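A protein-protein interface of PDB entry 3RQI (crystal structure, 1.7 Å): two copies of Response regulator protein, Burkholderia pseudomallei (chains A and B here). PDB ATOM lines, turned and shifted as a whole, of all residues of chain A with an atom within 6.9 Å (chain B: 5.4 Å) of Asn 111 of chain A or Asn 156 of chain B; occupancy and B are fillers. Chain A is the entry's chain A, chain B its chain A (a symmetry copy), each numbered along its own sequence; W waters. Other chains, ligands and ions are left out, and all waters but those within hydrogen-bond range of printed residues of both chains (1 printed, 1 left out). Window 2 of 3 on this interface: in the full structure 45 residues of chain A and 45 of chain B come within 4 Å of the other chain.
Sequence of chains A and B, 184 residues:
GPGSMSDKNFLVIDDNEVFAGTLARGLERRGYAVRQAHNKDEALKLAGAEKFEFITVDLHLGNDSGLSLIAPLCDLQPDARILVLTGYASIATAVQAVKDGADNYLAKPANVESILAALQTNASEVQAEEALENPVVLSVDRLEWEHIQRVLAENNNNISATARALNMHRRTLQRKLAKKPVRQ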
ATOM      1  N   LEU A  23      22.323 -20.860 -29.979  1.00  0.00           N
ATOM      2  CA  LEU A  23      21.595 -21.057 -28.730  1.00  0.00           C
ATOM      3  C   LEU A  23      21.065 -22.491 -28.671  1.00  0.00           C
ATOM      4  O   LEU A  23      21.219 -23.163 -27.656  1.00  0.00           O
ATOM      5  CB  LEU A  23      20.476 -20.012 -28.597  1.00  0.00           C
ATOM      6  CG  LEU A  23      19.485 -20.218 -27.443  1.00  0.00           C
ATOM      7  CD1 LEU A  23      20.212 -20.319 -26.087  1.00  0.00           C
ATOM      8  CD2 LEU A  23      18.470 -19.044 -27.428  1.00  0.00           C
ATOM      9  N   ARG A  30      23.114 -29.442 -23.226  1.00  0.00           N
ATOM     10  CA  ARG A  30      22.620 -29.548 -21.854  1.00  0.00           C
ATOM     11  C   ARG A  30      21.401 -30.457 -21.757  1.00  0.00           C
ATOM     12  O   ARG A  30      20.733 -30.537 -20.718  1.00  0.00           O
ATOM     13  CB  ARG A  30      22.320 -28.157 -21.301  1.00  0.00           C
ATOM     14  CG  ARG A  30      23.579 -27.407 -20.944  1.00  0.00           C
ATOM     15  CD  ARG A  30      23.409 -25.903 -20.966  1.00  0.00           C
ATOM     16  NE  ARG A  30      24.672 -25.228 -20.645  1.00  0.00           N
ATOM     17  CZ  ARG A  30      25.634 -24.923 -21.519  1.00  0.00           C
ATOM     18  NH1 ARG A  30      25.522 -25.196 -22.821  1.00  0.00           N
ATOM     19  NH2 ARG A  30      26.734 -24.325 -21.080  1.00  0.00           N
ATOM     20  N   LEU A 106      15.277 -10.777 -20.457  1.00  0.00           N
ATOM     21  CA  LEU A 106      16.746 -10.616 -20.428  1.00  0.00           C
ATOM     22  C   LEU A 106      17.266  -9.904 -21.662  1.00  0.00           C
ATOM     23  O   LEU A 106      16.799 -10.136 -22.794  1.00  0.00           O
ATOM     24  CB  LEU A 106      17.421 -11.979 -20.388  1.00  0.00           C
ATOM     25  CG  LEU A 106      17.639 -12.759 -19.098  1.00  0.00           C
ATOM     26  CD1 LEU A 106      18.629 -13.876 -19.505  1.00  0.00           C
ATOM     27  CD2 LEU A 106      18.209 -11.869 -17.999  1.00  0.00           C
ATOM     28  N   ALA A 107      18.211  -8.989 -21.430  1.00  0.00           N
ATOM     29  CA  ALA A 107      18.956  -8.382 -22.543  1.00  0.00           C
ATOM     30  C   ALA A 107      20.000  -9.321 -23.135  1.00  0.00           C
ATOM     31  O   ALA A 107      20.739 -10.006 -22.390  1.00  0.00           O
ATOM     32  CB  ALA A 107      19.633  -7.086 -22.072  1.00  0.00           C
ATOM     33  N   PRO A 109      23.634  -9.492 -24.896  1.00  0.00           N
ATOM     34  CA  PRO A 109      23.958 -10.906 -24.961  1.00  0.00           C
ATOM     35  C   PRO A 109      23.827 -11.575 -23.588  1.00  0.00           C
ATOM     36  O   PRO A 109      24.081 -10.956 -22.540  1.00  0.00           O
ATOM     37  CB  PRO A 109      25.436 -10.915 -25.444  1.00  0.00           C
ATOM     38  CG  PRO A 109      25.965  -9.697 -24.990  1.00  0.00           C
ATOM     39  CD  PRO A 109      24.860  -8.666 -24.890  1.00  0.00           C
ATOM     40  N   ALA A 110      23.389 -12.823 -23.624  1.00  0.00           N
ATOM     41  CA  ALA A 110      23.264 -13.648 -22.424  1.00  0.00           C
ATOM     42  C   ALA A 110      23.828 -14.997 -22.803  1.00  0.00           C
ATOM     43  O   ALA A 110      23.755 -15.380 -23.972  1.00  0.00           O
ATOM     44  CB  ALA A 110      21.770 -13.786 -22.025  1.00  0.00           C
ATOM     45  N   ASN A 111      24.402 -15.719 -21.845  1.00  0.00           N
ATOM     46  CA  ASN A 111      24.852 -17.077 -22.119  1.00  0.00           C
ATOM     47  C   ASN A 111      23.790 -18.089 -21.754  1.00  0.00           C
ATOM     48  O   ASN A 111      22.772 -17.753 -21.139  1.00  0.00           O
ATOM     49  CB  ASN A 111      26.225 -17.393 -21.457  1.00  0.00           C
ATOM     50  CG  ASN A 111      26.216 -17.246 -19.937  1.00  0.00           C
ATOM     51  OD1 ASN A 111      25.279 -17.650 -19.248  1.00  0.00           O
ATOM     52  ND2 ASN A 111      27.303 -16.707 -19.401  1.00  0.00           N
ATOM     53  N   VAL A 112      24.020 -19.333 -22.148  1.00  0.00           N
ATOM     54  CA  VAL A 112      23.037 -20.383 -21.954  1.00  0.00           C
ATOM     55  C   VAL A 112      22.692 -20.582 -20.464  1.00  0.00           C
ATOM     56  O   VAL A 112      21.498 -20.691 -20.120  1.00  0.00           O
ATOM     57  CB  VAL A 112      23.466 -21.716 -22.611  1.00  0.00           C
ATOM     58  CG1 VAL A 112      22.453 -22.821 -22.263  1.00  0.00           C
ATOM     59  CG2 VAL A 112      23.546 -21.556 -24.150  1.00  0.00           C
ATOM     60  N   GLU A 113      23.709 -20.629 -19.597  1.00  0.00           N
ATOM     61  CA  GLU A 113      23.479 -20.711 -18.134  1.00  0.00           C
ATOM     62  C   GLU A 113      22.558 -19.608 -17.597  1.00  0.00           C
ATOM     63  O   GLU A 113      21.646 -19.885 -16.805  1.00  0.00           O
ATOM     64  CB  GLU A 113      24.810 -20.744 -17.342  1.00  0.00           C
ATOM     65  N   SER A 114      22.760 -18.371 -18.047  1.00  0.00           N
ATOM     66  CA  SER A 114      21.948 -17.260 -17.538  1.00  0.00           C
ATOM     67  C   SER A 114      20.526 -17.275 -18.107  1.00  0.00           C
ATOM     68  O   SER A 114      19.572 -16.865 -17.440  1.00  0.00           O
ATOM     69  CB  SER A 114      22.632 -15.928 -17.751  1.00  0.00           C
ATOM     70  OG  SER A 114      22.608 -15.521 -19.080  1.00  0.00           O
ATOM     71  N   ILE A 115      20.408 -17.782 -19.331  1.00  0.00           N
ATOM     72  CA  ILE A 115      19.087 -17.939 -19.965  1.00  0.00           C
ATOM     73  C   ILE A 115      18.302 -18.974 -19.162  1.00  0.00           C
ATOM     74  O   ILE A 115      17.173 -18.702 -18.763  1.00  0.00           O
ATOM     75  CB  ILE A 115      19.215 -18.344 -21.464  1.00  0.00           C
ATOM     76  CG1 ILE A 115      19.661 -17.128 -22.264  1.00  0.00           C
ATOM     77  CG2 ILE A 115      17.849 -18.866 -22.040  1.00  0.00           C
ATOM     78  CD1 ILE A 115      20.114 -17.466 -23.651  1.00  0.00           C
ATOM     79  N   LEU A 116      18.913 -20.144 -18.888  1.00  0.00           N
ATOM     80  CA  LEU A 116      18.270 -21.153 -18.037  1.00  0.00           C
ATOM     81  C   LEU A 116      17.930 -20.615 -16.638  1.00  0.00           C
ATOM     82  O   LEU A 116      16.826 -20.873 -16.129  1.00  0.00           O
ATOM     83  CB  LEU A 116      19.111 -22.446 -17.971  1.00  0.00           C
ATOM     84  CG  LEU A 116      19.165 -23.224 -19.303  1.00  0.00           C
ATOM     85  CD1 LEU A 116      20.238 -24.348 -19.293  1.00  0.00           C
ATOM     86  CD2 LEU A 116      17.796 -23.798 -19.728  1.00  0.00           C
ATOM     87  N   ALA A 117      18.867 -19.878 -16.020  1.00  0.00           N
ATOM     88  CA  ALA A 117      18.628 -19.274 -14.693  1.00  0.00           C
ATOM     89  C   ALA A 117      17.384 -18.378 -14.699  1.00  0.00           C
ATOM     90  O   ALA A 117      16.526 -18.443 -13.787  1.00  0.00           O
ATOM     91  CB  ALA A 117      19.890 -18.468 -14.222  1.00  0.00           C
ATOM     92  N   LEU B 152      33.201  -8.597 -20.626  1.00  0.00           N
ATOM     93  CA  LEU B 152      32.130  -9.424 -21.199  1.00  0.00           C
ATOM     94  C   LEU B 152      32.624 -10.855 -21.451  1.00  0.00           C
ATOM     95  O   LEU B 152      31.917 -11.823 -21.156  1.00  0.00           O
ATOM     96  CB  LEU B 152      31.589  -8.789 -22.494  1.00  0.00           C
ATOM     97  CG  LEU B 152      30.362  -9.381 -23.204  1.00  0.00           C
ATOM     98  CD1 LEU B 152      29.084  -9.199 -22.386  1.00  0.00           C
ATOM     99  CD2 LEU B 152      30.197  -8.759 -24.582  1.00  0.00           C
ATOM    100  N   ALA B 153      33.844 -10.975 -21.978  1.00  0.00           N
ATOM    101  CA  ALA B 153      34.479 -12.279 -22.230  1.00  0.00           C
ATOM    102  C   ALA B 153      34.828 -13.024 -20.933  1.00  0.00           C
ATOM    103  O   ALA B 153      34.738 -14.251 -20.873  1.00  0.00           O
ATOM    104  CB  ALA B 153      35.732 -12.108 -23.104  1.00  0.00           C
ATOM    105  N   GLU B 154      35.234 -12.268 -19.913  1.00  0.00           N
ATOM    106  CA  GLU B 154      35.545 -12.801 -18.579  1.00  0.00           C
ATOM    107  C   GLU B 154      34.296 -13.267 -17.828  1.00  0.00           C
ATOM    108  O   GLU B 154      34.390 -13.989 -16.829  1.00  0.00           O
ATOM    109  CB  GLU B 154      36.273 -11.747 -17.739  1.00  0.00           C
ATOM    110  N   ASN B 155      33.134 -12.837 -18.314  1.00  0.00           N
ATOM    111  CA  ASN B 155      31.858 -13.203 -17.716  1.00  0.00           C
ATOM    112  C   ASN B 155      31.044 -14.172 -18.585  1.00  0.00           C
ATOM    113  O   ASN B 155      29.832 -14.295 -18.413  1.00  0.00           O
ATOM    114  CB  ASN B 155      31.063 -11.940 -17.375  1.00  0.00           C
ATOM    115  CG  ASN B 155      31.580 -11.251 -16.120  1.00  0.00           C
ATOM    116  OD1 ASN B 155      31.334 -11.708 -15.002  1.00  0.00           O
ATOM    117  ND2 ASN B 155      32.291 -10.149 -16.298  1.00  0.00           N
ATOM    118  N   ASN B 156      31.739 -14.870 -19.488  1.00  0.00           N
ATOM    119  CA  ASN B 156      31.144 -15.833 -20.434  1.00  0.00           C
ATOM    120  C   ASN B 156      30.068 -15.214 -21.351  1.00  0.00           C
ATOM    121  O   ASN B 156      29.026 -15.827 -21.609  1.00  0.00           O
ATOM    122  CB  ASN B 156      30.638 -17.095 -19.698  1.00  0.00           C
ATOM    123  CG  ASN B 156      30.328 -18.266 -20.645  1.00  0.00           C
ATOM    124  OD1 ASN B 156      30.714 -18.267 -21.817  1.00  0.00           O
ATOM    125  ND2 ASN B 156      29.624 -19.271 -20.128  1.00  0.00           N
ATOM    126  N   ASN B 157      30.348 -14.004 -21.845  1.00  0.00           N
ATOM    127  CA  ASN B 157      29.447 -13.247 -22.741  1.00  0.00           C
ATOM    128  C   ASN B 157      28.071 -12.920 -22.120  1.00  0.00           C
ATOM    129  O   ASN B 157      27.053 -12.865 -22.809  1.00  0.00           O
ATOM    130  CB  ASN B 157      29.314 -13.940 -24.113  1.00  0.00           C
ATOM    131  CG  ASN B 157      28.918 -12.977 -25.230  1.00  0.00           C
ATOM    132  OD1 ASN B 157      29.253 -11.795 -25.201  1.00  0.00           O
ATOM    133  ND2 ASN B 157      28.200 -13.494 -26.229  1.00  0.00           N
ATOM    134  N   ASN B 158      28.084 -12.681 -20.812  1.00  0.00           N
ATOM    135  CA  ASN B 158      26.895 -12.369 -20.024  1.00  0.00           C
ATOM    136  C   ASN B 158      26.774 -10.872 -19.695  1.00  0.00           C
ATOM    137  O   ASN B 158      27.501 -10.347 -18.840  1.00  0.00           O
ATOM    138  CB  ASN B 158      26.937 -13.202 -18.738  1.00  0.00           C
ATOM    139  CG  ASN B 158      25.651 -13.145 -17.952  1.00  0.00           C
ATOM    140  OD1 ASN B 158      24.711 -12.428 -18.306  1.00  0.00           O
ATOM    141  ND2 ASN B 158      25.602 -13.903 -16.863  1.00  0.00           N
HETATM  142  O   HOH W   1      26.588 -20.841 -20.156  1.00  0.00           O
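No position is printed for both chains.
Of the printed residues of chain B, Ala 110 of chain A touches Asn 157 (3.8 Å). Printed residues of chain B within 4 Å of Asn 111 of chain A: Asn 155, Asn 156 and Asn 158. Val 112 of chain A touches none of the printed residues of chain B. Of the printed residues of chain A, Asn 155 of chain B touches Asn 111 (3.6 Å). Of the printed residues of chain A, Asn 157 of chain B touches Pro 109 (3.5 Å) and Ala 110 (3.8 Å). The nearest printed residue of chain B that does not touch Asn 111 of chain A is Asn 157 of chain B (4.01 Å). The nearest residue of chain A that does not touch Asn 156 of chain B is Ala 110 of chain A (5.4 Å). The nearest printed residue of chain A that does not touch Asn 155 of chain B is Ser 114 of chain A (7.4 Å).
Water W1 lies within hydrogen-bond range of N of Glu 113 of chain A and ND2 of Asn 156 of chain B.
ND2 of Asn 111 of chain A is in hydrogen-bond range of O of Asn 156 of chain B (2.9 Å).
Of the 7 printed residues of chain B, 4 touch a printed residue of chain A. Printed residues of chain B that touch a printed residue of chain A: Asn 155, Asn 156, Asn 157 and Asn 158. Of the 13 printed residues of chain A, 4 touch a printed residue of chain B. Hydrophobic or aromatic side chains of chain A that line the printed part of chain B: Pro 109. Among the printed residues, no Asp or Glu carboxylate lies within 4 Å of a Lys or Arg side-chain nitrogen of the other chain.
The side-chain amide oxygen (OD1) of Asn 111 of chain A sits close to the backbone NH (N) of Glu 113 of chain A (3.4 Å). The side-chain amide oxygen (OD1) of Asn 111 of chain A is in hydrogen-bond range of the backbone NH (N) of Ser 114 of chain A (2.9 Å). The backbone NH of Asn 157 of chain B lies within hydrogen-bond range of the backbone carbonyl oxygen of Leu 152 of chain B (2.8 Å).
Among the printed residues, pairs that only touch across the chains: Pro 109 of chain A with Asn 157 of chain B, Asn 111 of chain A with Asn 158 of chain B, Asn 111 of chain A with Asn 155 of chain B, Ser 114 of chain A with Asn 158 of chain B, Ala 110 of chain A with Asn 157 of chain B and Pro 109 of chain A with Asn 158 of chain B.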
